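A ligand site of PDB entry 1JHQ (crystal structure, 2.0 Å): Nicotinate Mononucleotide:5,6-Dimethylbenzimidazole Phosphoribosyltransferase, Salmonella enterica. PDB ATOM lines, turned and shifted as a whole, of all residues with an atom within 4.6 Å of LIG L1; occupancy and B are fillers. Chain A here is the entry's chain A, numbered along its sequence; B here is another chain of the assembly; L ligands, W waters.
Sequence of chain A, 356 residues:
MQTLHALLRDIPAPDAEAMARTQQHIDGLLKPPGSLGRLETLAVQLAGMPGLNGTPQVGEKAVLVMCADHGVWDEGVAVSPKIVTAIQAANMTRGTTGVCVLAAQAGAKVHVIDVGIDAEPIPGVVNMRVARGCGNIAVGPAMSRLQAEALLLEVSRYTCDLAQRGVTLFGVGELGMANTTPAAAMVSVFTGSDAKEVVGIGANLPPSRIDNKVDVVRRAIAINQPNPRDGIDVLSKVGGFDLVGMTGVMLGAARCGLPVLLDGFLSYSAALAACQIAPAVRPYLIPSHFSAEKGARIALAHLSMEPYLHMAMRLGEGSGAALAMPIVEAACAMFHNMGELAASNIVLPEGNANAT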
ATOM      1  N   VAL A  77     -17.486 -23.806  24.095  1.00  0.00           N
ATOM      2  CA  VAL A  77     -16.365 -23.819  23.159  1.00  0.00           C
ATOM      3  C   VAL A  77     -16.251 -22.560  22.283  1.00  0.00           C
ATOM      4  O   VAL A  77     -15.298 -22.438  21.497  1.00  0.00           O
ATOM      5  CB  VAL A  77     -16.348 -25.068  22.278  1.00  0.00           C
ATOM      6  CG1 VAL A  77     -16.170 -26.327  23.131  1.00  0.00           C
ATOM      7  CG2 VAL A  77     -17.655 -25.131  21.490  1.00  0.00           C
ATOM      8  N   ALA A  78     -17.212 -21.639  22.405  1.00  0.00           N
ATOM      9  CA  ALA A  78     -17.229 -20.382  21.604  1.00  0.00           C
ATOM     10  C   ALA A  78     -17.640 -19.126  22.413  1.00  0.00           C
ATOM     11  O   ALA A  78     -18.633 -19.122  23.118  1.00  0.00           O
ATOM     12  CB  ALA A  78     -18.150 -20.543  20.401  1.00  0.00           C
ATOM     13  N   SER A  80     -18.466 -16.116  21.036  1.00  0.00           N
ATOM     14  CA  SER A  80     -19.443 -15.290  20.344  1.00  0.00           C
ATOM     15  C   SER A  80     -20.846 -15.737  20.779  1.00  0.00           C
ATOM     16  O   SER A  80     -21.140 -16.927  20.813  1.00  0.00           O
ATOM     17  CB  SER A  80     -19.403 -15.473  18.822  1.00  0.00           C
ATOM     18  OG  SER A  80     -18.143 -15.101  18.290  1.00  0.00           O
ATOM     19  N   VAL A  84     -25.312 -14.392  17.222  1.00  0.00           N
ATOM     20  CA  VAL A  84     -24.488 -13.791  16.195  1.00  0.00           C
ATOM     21  C   VAL A  84     -24.706 -14.455  14.824  1.00  0.00           C
ATOM     22  O   VAL A  84     -24.633 -13.803  13.793  1.00  0.00           O
ATOM     23  CB  VAL A  84     -23.011 -13.697  16.615  1.00  0.00           C
ATOM     24  CG1 VAL A  84     -22.150 -13.050  15.537  1.00  0.00           C
ATOM     25  CG2 VAL A  84     -22.887 -12.904  17.914  1.00  0.00           C
ATOM     26  N   GLN A  88     -25.563 -11.958  11.906  1.00  0.00           N
ATOM     27  CA  GLN A  88     -24.585 -11.848  10.859  1.00  0.00           C
ATOM     28  C   GLN A  88     -25.162 -12.345   9.521  1.00  0.00           C
ATOM     29  O   GLN A  88     -24.905 -11.798   8.428  1.00  0.00           O
ATOM     30  CB  GLN A  88     -23.260 -12.524  11.305  1.00  0.00           C
ATOM     31  CG  GLN A  88     -22.072 -12.267  10.352  1.00  0.00           C
ATOM     32  CD  GLN A  88     -21.506 -10.862  10.430  1.00  0.00           C
ATOM     33  OE1 GLN A  88     -22.206  -9.907  10.838  1.00  0.00           O
ATOM     34  NE2 GLN A  88     -20.256 -10.706  10.035  1.00  0.00           N
ATOM     35  N   GLU A 174     -19.000 -20.236   5.182  1.00  0.00           N
ATOM     36  CA  GLU A 174     -19.901 -20.606   6.260  1.00  0.00           C
ATOM     37  C   GLU A 174     -20.071 -19.495   7.286  1.00  0.00           C
ATOM     38  O   GLU A 174     -19.433 -18.434   7.204  1.00  0.00           O
ATOM     39  CB  GLU A 174     -19.432 -21.900   6.964  1.00  0.00           C
ATOM     40  CG  GLU A 174     -17.910 -21.919   7.327  1.00  0.00           C
ATOM     41  CD  GLU A 174     -17.472 -20.690   8.125  1.00  0.00           C
ATOM     42  OE1 GLU A 174     -17.868 -20.442   9.240  1.00  0.00           O
ATOM     43  OE2 GLU A 174     -16.695 -19.874   7.428  1.00  0.00           O
ATOM     44  N   LEU A 175     -20.953 -19.783   8.243  1.00  0.00           N
ATOM     45  CA  LEU A 175     -21.312 -18.929   9.368  1.00  0.00           C
ATOM     46  C   LEU A 175     -21.985 -19.814  10.410  1.00  0.00           C
ATOM     47  O   LEU A 175     -22.990 -20.444  10.126  1.00  0.00           O
ATOM     48  CB  LEU A 175     -22.251 -17.778   8.913  1.00  0.00           C
ATOM     49  CG  LEU A 175     -22.398 -16.585   9.849  1.00  0.00           C
ATOM     50  CD1 LEU A 175     -21.039 -15.871  10.051  1.00  0.00           C
ATOM     51  CD2 LEU A 175     -23.436 -15.627   9.252  1.00  0.00           C
ATOM     52  N   GLY A 176     -21.404 -19.912  11.590  1.00  0.00           N
ATOM     53  CA  GLY A 176     -21.972 -20.757  12.623  1.00  0.00           C
ATOM     54  C   GLY A 176     -21.096 -20.713  13.850  1.00  0.00           C
ATOM     55  O   GLY A 176     -19.996 -21.292  13.864  1.00  0.00           O
ATOM     56  N   MET A 177     -21.580 -19.992  14.872  1.00  0.00           N
ATOM     57  CA  MET A 177     -20.826 -19.859  16.109  1.00  0.00           C
ATOM     58  C   MET A 177     -20.568 -21.265  16.627  1.00  0.00           C
ATOM     59  O   MET A 177     -21.493 -22.080  16.613  1.00  0.00           O
ATOM     60  CB  MET A 177     -21.572 -18.998  17.154  1.00  0.00           C
ATOM     61  CG  MET A 177     -22.004 -17.630  16.614  1.00  0.00           C
ATOM     62  SD  MET A 177     -20.634 -16.720  15.809  1.00  0.00           S
ATOM     63  CE  MET A 177     -21.276 -16.499  14.108  1.00  0.00           C
ATOM     64  N   ALA A 178     -19.325 -21.540  17.029  1.00  0.00           N
ATOM     65  CA  ALA A 178     -18.875 -22.847  17.539  1.00  0.00           C
ATOM     66  C   ALA A 178     -18.465 -23.854  16.454  1.00  0.00           C
ATOM     67  O   ALA A 178     -17.993 -24.970  16.749  1.00  0.00           O
ATOM     68  CB  ALA A 178     -19.861 -23.482  18.516  1.00  0.00           C
ATOM     69  N   ASN A 179     -18.587 -23.468  15.171  1.00  0.00           N
ATOM     70  CA  ASN A 179     -18.245 -24.383  14.076  1.00  0.00           C
ATOM     71  C   ASN A 179     -16.814 -24.914  13.980  1.00  0.00           C
ATOM     72  O   ASN A 179     -16.566 -25.951  13.345  1.00  0.00           O
ATOM     73  CB  ASN A 179     -18.920 -24.021  12.723  1.00  0.00           C
ATOM     74  CG  ASN A 179     -18.309 -22.832  11.994  1.00  0.00           C
ATOM     75  OD1 ASN A 179     -17.293 -22.260  12.445  1.00  0.00           O
ATOM     76  ND2 ASN A 179     -18.918 -22.470  10.861  1.00  0.00           N
ATOM     77  N   THR A 180     -15.843 -24.224  14.604  1.00  0.00           N
ATOM     78  CA  THR A 180     -14.459 -24.679  14.568  1.00  0.00           C
ATOM     79  C   THR A 180     -14.256 -25.945  15.403  1.00  0.00           C
ATOM     80  O   THR A 180     -13.278 -26.704  15.244  1.00  0.00           O
ATOM     81  CB  THR A 180     -13.420 -23.556  14.842  1.00  0.00           C
ATOM     82  OG1 THR A 180     -13.513 -23.105  16.185  1.00  0.00           O
ATOM     83  CG2 THR A 180     -13.650 -22.373  13.914  1.00  0.00           C
ATOM     84  N   THR A 181     -15.235 -26.215  16.269  1.00  0.00           N
ATOM     85  CA  THR A 181     -15.169 -27.407  17.080  1.00  0.00           C
ATOM     86  C   THR A 181     -15.430 -28.681  16.234  1.00  0.00           C
ATOM     87  O   THR A 181     -14.576 -29.533  16.123  1.00  0.00           O
ATOM     88  CB  THR A 181     -16.042 -27.250  18.320  1.00  0.00           C
ATOM     89  OG1 THR A 181     -15.429 -26.262  19.110  1.00  0.00           O
ATOM     90  CG2 THR A 181     -16.108 -28.574  19.073  1.00  0.00           C
ATOM     91  N   ILE A 201      -8.002 -21.573  18.284  1.00  0.00           N
ATOM     92  CA  ILE A 201      -8.728 -20.588  19.066  1.00  0.00           C
ATOM     93  C   ILE A 201     -10.029 -20.119  18.397  1.00  0.00           C
ATOM     94  O   ILE A 201     -10.813 -19.353  18.982  1.00  0.00           O
ATOM     95  CB  ILE A 201      -7.825 -19.421  19.523  1.00  0.00           C
ATOM     96  N   GLY A 202     -10.257 -20.560  17.156  1.00  0.00           N
ATOM     97  CA  GLY A 202     -11.471 -20.134  16.471  1.00  0.00           C
ATOM     98  C   GLY A 202     -11.622 -18.594  16.465  1.00  0.00           C
ATOM     99  O   GLY A 202     -10.702 -17.813  16.156  1.00  0.00           O
ATOM    100  N   ALA A 203     -12.805 -18.144  16.817  1.00  0.00           N
ATOM    101  CA  ALA A 203     -13.078 -16.714  16.837  1.00  0.00           C
ATOM    102  C   ALA A 203     -12.675 -16.134  18.184  1.00  0.00           C
ATOM    103  O   ALA A 203     -13.506 -15.787  19.019  1.00  0.00           O
ATOM    104  CB  ALA A 203     -14.529 -16.376  16.482  1.00  0.00           C
ATOM    105  N   LYS A 213     -12.115 -27.070  25.041  1.00  0.00           N
ATOM    106  CA  LYS A 213     -12.436 -27.352  23.649  1.00  0.00           C
ATOM    107  C   LYS A 213     -11.818 -28.683  23.205  1.00  0.00           C
ATOM    108  O   LYS A 213     -12.451 -29.485  22.500  1.00  0.00           O
ATOM    109  CB  LYS A 213     -12.011 -26.204  22.761  1.00  0.00           C
ATOM    110  CG  LYS A 213     -12.422 -26.305  21.308  1.00  0.00           C
ATOM    111  CD  LYS A 213     -12.219 -24.943  20.637  1.00  0.00           C
ATOM    112  CE  LYS A 213     -12.381 -24.909  19.130  1.00  0.00           C
ATOM    113  NZ  LYS A 213     -12.040 -23.572  18.571  1.00  0.00           N
ATOM    114  N   LEU A 315     -11.283 -15.414   9.511  1.00  0.00           N
ATOM    115  CA  LEU A 315     -12.612 -14.906   9.613  1.00  0.00           C
ATOM    116  C   LEU A 315     -13.667 -15.925   9.151  1.00  0.00           C
ATOM    117  O   LEU A 315     -14.756 -16.002   9.735  1.00  0.00           O
ATOM    118  CB  LEU A 315     -12.768 -13.597   8.786  1.00  0.00           C
ATOM    119  CG  LEU A 315     -14.206 -13.025   8.655  1.00  0.00           C
ATOM    120  CD1 LEU A 315     -14.761 -12.664  10.032  1.00  0.00           C
ATOM    121  CD2 LEU A 315     -14.191 -11.756   7.775  1.00  0.00           C
ATOM    122  N   GLY A 316     -13.379 -16.643   8.062  1.00  0.00           N
ATOM    123  CA  GLY A 316     -14.380 -17.535   7.505  1.00  0.00           C
ATOM    124  C   GLY A 316     -15.295 -16.709   6.594  1.00  0.00           C
ATOM    125  O   GLY A 316     -14.885 -15.652   6.034  1.00  0.00           O
ATOM    126  N   GLU A 317     -16.540 -17.179   6.438  1.00  0.00           N
ATOM    127  CA  GLU A 317     -17.575 -16.542   5.599  1.00  0.00           C
ATOM    128  C   GLU A 317     -17.329 -16.711   4.113  1.00  0.00           C
ATOM    129  O   GLU A 317     -18.165 -16.328   3.298  1.00  0.00           O
ATOM    130  CB  GLU A 317     -17.661 -15.017   5.852  1.00  0.00           C
ATOM    131  CG  GLU A 317     -17.765 -14.628   7.345  1.00  0.00           C
ATOM    132  CD  GLU A 317     -18.083 -13.166   7.506  1.00  0.00           C
ATOM    133  OE1 GLU A 317     -18.111 -12.395   6.566  1.00  0.00           O
ATOM    134  OE2 GLU A 317     -18.357 -12.812   8.737  1.00  0.00           O
ATOM    135  N   LEU B  30     -17.477  -5.306  11.718  1.00  0.00           N
ATOM    136  CA  LEU B  30     -18.353  -6.486  11.861  1.00  0.00           C
ATOM    137  C   LEU B  30     -17.620  -7.841  11.756  1.00  0.00           C
ATOM    138  O   LEU B  30     -17.907  -8.625  10.839  1.00  0.00           O
ATOM    139  CB  LEU B  30     -19.351  -6.366  10.705  1.00  0.00           C
ATOM    140  CG  LEU B  30     -20.811  -6.624  10.978  1.00  0.00           C
ATOM    141  CD1 LEU B  30     -21.234  -6.274  12.411  1.00  0.00           C
ATOM    142  CD2 LEU B  30     -21.596  -5.816   9.953  1.00  0.00           C
ATOM    143  N   LYS B  31     -16.712  -8.138  12.686  1.00  0.00           N
ATOM    144  CA  LYS B  31     -15.931  -9.381  12.661  1.00  0.00           C
ATOM    145  C   LYS B  31     -15.210  -9.490  13.981  1.00  0.00           C
ATOM    146  O   LYS B  31     -15.042  -8.496  14.683  1.00  0.00           O
ATOM    147  CB  LYS B  31     -14.818  -9.280  11.595  1.00  0.00           C
ATOM    148  CG  LYS B  31     -13.860  -8.114  11.878  1.00  0.00           C
ATOM    149  CD  LYS B  31     -12.695  -7.943  10.899  1.00  0.00           C
ATOM    150  CE  LYS B  31     -12.000  -6.592  11.086  1.00  0.00           C
ATOM    151  NZ  LYS B  31     -11.238  -6.483  12.344  1.00  0.00           N
ATOM    152  N   PRO B  32     -14.731 -10.676  14.287  1.00  0.00           N
ATOM    153  CA  PRO B  32     -13.942 -10.823  15.509  1.00  0.00           C
ATOM    154  C   PRO B  32     -12.654 -10.003  15.351  1.00  0.00           C
ATOM    155  O   PRO B  32     -11.990 -10.044  14.307  1.00  0.00           O
ATOM    156  CB  PRO B  32     -13.603 -12.321  15.637  1.00  0.00           C
ATOM    157  CG  PRO B  32     -14.452 -13.040  14.586  1.00  0.00           C
ATOM    158  CD  PRO B  32     -15.109 -11.993  13.697  1.00  0.00           C
ATOM    159  N   LEU B 341     -19.799  -3.445  14.391  1.00  0.00           N
ATOM    160  CA  LEU B 341     -20.337  -4.249  15.432  1.00  0.00           C
ATOM    161  C   LEU B 341     -21.437  -3.532  16.203  1.00  0.00           C
ATOM    162  O   LEU B 341     -22.531  -4.051  16.430  1.00  0.00           O
ATOM    163  CB  LEU B 341     -19.226  -4.658  16.418  1.00  0.00           C
ATOM    164  CG  LEU B 341     -18.244  -5.668  15.831  1.00  0.00           C
ATOM    165  CD1 LEU B 341     -17.029  -5.810  16.753  1.00  0.00           C
ATOM    166  CD2 LEU B 341     -18.944  -7.032  15.654  1.00  0.00           C
ATOM    167  N   ILE B 346     -23.933  -5.923  18.451  1.00  0.00           N
ATOM    168  CA  ILE B 346     -23.100  -7.084  18.706  1.00  0.00           C
ATOM    169  C   ILE B 346     -21.949  -6.737  19.617  1.00  0.00           C
ATOM    170  O   ILE B 346     -21.249  -5.756  19.398  1.00  0.00           O
ATOM    171  CB  ILE B 346     -22.588  -7.750  17.433  1.00  0.00           C
ATOM    172  CG1 ILE B 346     -23.751  -8.265  16.603  1.00  0.00           C
ATOM    173  CG2 ILE B 346     -21.670  -8.927  17.796  1.00  0.00           C
ATOM    174  CD1 ILE B 346     -23.335  -8.719  15.198  1.00  0.00           C
ATOM    175  N   LEU B 348     -18.504  -8.456  21.278  1.00  0.00           N
ATOM    176  CA  LEU B 348     -17.586  -9.578  21.367  1.00  0.00           C
ATOM    177  C   LEU B 348     -16.400  -9.175  22.237  1.00  0.00           C
ATOM    178  O   LEU B 348     -15.979  -8.012  22.179  1.00  0.00           O
ATOM    179  CB  LEU B 348     -17.048 -10.035  19.983  1.00  0.00           C
ATOM    180  CG  LEU B 348     -18.096 -10.150  18.881  1.00  0.00           C
ATOM    181  CD1 LEU B 348     -17.416 -10.244  17.507  1.00  0.00           C
ATOM    182  CD2 LEU B 348     -18.983 -11.372  19.121  1.00  0.00           C
HETATM  183  N1  LIG L   1     -17.943 -14.377  10.715  1.00  0.00           N
HETATM  184  N2  LIG L   1     -17.072 -16.037  11.976  1.00  0.00           N
HETATM  185  C1  LIG L   1     -17.317 -15.558  10.728  1.00  0.00           C
HETATM  186  C2  LIG L   1     -17.623 -15.029  12.820  1.00  0.00           C
HETATM  187  C3  LIG L   1     -18.123 -14.012  12.033  1.00  0.00           C
HETATM  188  C4  LIG L   1     -18.668 -12.859  12.614  1.00  0.00           C
HETATM  189  C5  LIG L   1     -18.773 -12.751  13.986  1.00  0.00           C
HETATM  190  C6  LIG L   1     -18.247 -13.790  14.794  1.00  0.00           C
HETATM  191  C7  LIG L   1     -17.700 -14.921  14.214  1.00  0.00           C
HETATM  192  O1  LIG L   1     -19.249 -11.705  14.745  1.00  0.00           O
HETATM  193  C8  LIG L   1     -19.669 -10.626  13.929  1.00  0.00           C
HETATM  194  P1  LIG L   1     -15.884 -20.351  16.798  1.00  0.00           P
HETATM  195  O2  LIG L   1     -15.707 -21.803  16.535  1.00  0.00           O
HETATM  196  O3  LIG L   1     -14.929 -19.877  17.825  1.00  0.00           O
HETATM  197  O4  LIG L   1     -17.268 -19.842  17.075  1.00  0.00           O
HETATM  198  O5  LIG L   1     -15.411 -19.727  15.371  1.00  0.00           O
HETATM  199  C9  LIG L   1     -16.149 -20.003  14.170  1.00  0.00           C
HETATM  200  C10 LIG L   1     -17.155 -18.878  13.947  1.00  0.00           C
HETATM  201  O6  LIG L   1     -16.430 -17.620  13.727  1.00  0.00           O
HETATM  202  C11 LIG L   1     -18.020 -19.054  12.700  1.00  0.00           C
HETATM  203  O7  LIG L   1     -19.187 -18.213  12.702  1.00  0.00           O
HETATM  204  C12 LIG L   1     -17.010 -18.542  11.662  1.00  0.00           C
HETATM  205  O8  LIG L   1     -17.745 -18.213  10.456  1.00  0.00           O
HETATM  206  C13 LIG L   1     -16.393 -17.307  12.334  1.00  0.00           C
HETATM  207  N1  LG2 L   2     -13.584 -18.790  11.642  1.00  0.00           N
HETATM  208  C1  LG2 L   2     -13.100 -19.161  10.428  1.00  0.00           C
HETATM  209  C2  LG2 L   2     -11.773 -19.546  10.326  1.00  0.00           C
HETATM  210  C3  LG2 L   2     -10.913 -19.588  11.483  1.00  0.00           C
HETATM  211  C4  LG2 L   2     -11.540 -19.187  12.671  1.00  0.00           C
HETATM  212  C5  LG2 L   2     -12.841 -18.790  12.829  1.00  0.00           C
HETATM  213  C6  LG2 L   2     -11.226 -19.947   8.972  1.00  0.00           C
HETATM  214  O1  LG2 L   2     -10.003 -20.300   8.876  1.00  0.00           O
HETATM  215  O2  LG2 L   2     -11.984 -19.943   7.953  1.00  0.00           O
HETATM  216  O   HOH W   1     -14.965 -18.375  20.110  1.00  0.00           O
HETATM  217  O   HOH W   2     -15.768 -23.541  18.788  1.00  0.00           O
HETATM  218  O   HOH W   3     -17.277 -17.801  18.726  1.00  0.00           O
HETATM  219  O   HOH W   4     -13.458 -21.386  19.453  1.00  0.00           O
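An oxygen (O8) of LIG L1 lies within hydrogen-bond range of the side-chain carboxylate of Glu 174 (2.5 Å). OE2 of Glu 317 lies within hydrogen-bond range of N1 of LIG L1 (2.6 Å). The backbone NH (N) of Thr 180 is in hydrogen-bond range of an oxygen (O2) of LIG L1 (3.1 Å). An oxygen (O2) of LIG L1 is in hydrogen-bond range of the side-chain hydroxyl (OG1) of Thr 180 (2.6 Å). The backbone NH (N) of Ala 178 is in hydrogen-bond range of an oxygen (O4) of LIG L1 (2.7 Å). The backbone NH (N) of Ala 203 is in hydrogen-bond range of an oxygen (O3) of LIG L1 (2.9 Å). The backbone NH (N) of Gly 176 sits at hydrogen-bond distance from an oxygen (O7) of LIG L1, 3.0 Å away. An oxygen (O7) of LIG L1 sits close to the backbone carbonyl oxygen (O) of Gly 176, at 3.4 Å. The side-chain sulfur (SD) of Met 177 sits close to an oxygen (O7) of LIG L1, at 3.7 Å.
The side-chain carboxylate (OE2) of Glu 174 is in hydrogen-bond range of the backbone NH (N) of Glu 317 (2.9 Å). The side-chain carboxylate (OE1) of Glu 174 sits at hydrogen-bond distance from the side-chain amide nitrogen (ND2) of Asn 179, 2.8 Å away. The side-chain amide nitrogen (NE2) of Gln 88 is in hydrogen-bond range of the side-chain carboxylate (OE2) of Glu 317, 3.1 Å away. The side-chain hydroxyl (OG1) of Thr 180 is in hydrogen-bond range of the side-chain amino group (NZ) of Lys 213. The side-chain amide oxygen (OD1) of Asn 179 lies close to the backbone carbonyl oxygen (O) of Gly 176 (3.2 Å). NE2 of Gln 88 lies within hydrogen-bond range of O of Leu 30 of chain B (3.2 Å).
A nitrogen (N2) of LIG L1 lies close to the backbone carbonyl oxygen (O) of Leu 315. Residues that only touch LIG L1: Ala 78 (3.5 Å), Ser 80 (3.7 Å), Val 84 (3.3 Å), Gln 88 (3.7 Å), Leu 175 (3.5 Å), Asn 179 (3.1 Å), Gly 202 (3.7 Å), Pro 32 of chain B (3.8 Å) and Leu 348 of chain B (3.6 Å). 17 residues have an atom within 4 Å of LIG L1: Ala 78, Ser 80, Val 84, Gln 88, Glu 174, Leu 175, Gly 176, Met 177, Ala 178, Asn 179, Thr 180, Gly 202, Ala 203, Leu 315, Glu 317, Pro 32 of chain B and Leu 348 of chain B. The nearest printed residue that does not touch LIG L1 is Leu 341 of chain B (4.1 Å).
Water W3 bridges O4 of LIG L1 and OG of Ser 80. Water W4 lies within hydrogen-bond range of an oxygen (O3) of LIG L1, the side-chain amino group (NZ) of Lys 213, the backbone carbonyl oxygen (O) of Val 77 and the backbone carbonyl oxygen (O) of Ile 201. Water W1 lies within hydrogen-bond range of O3 of LIG L1 (2.7 Å) and O of Ala 203 (3.2 Å). Water W2 lies within hydrogen-bond range of the side-chain hydroxyl (OG1) of Thr 181 (2.8 Å), an oxygen (O2) of LIG L1 (2.8 Å), the backbone carbonyl oxygen (O) of Val 77 (3.0 Å), the backbone carbonyl oxygen (O) of Ala 178 (3.3 Å) and the side-chain hydroxyl (OG1) of Thr 180 (3.5 Å).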
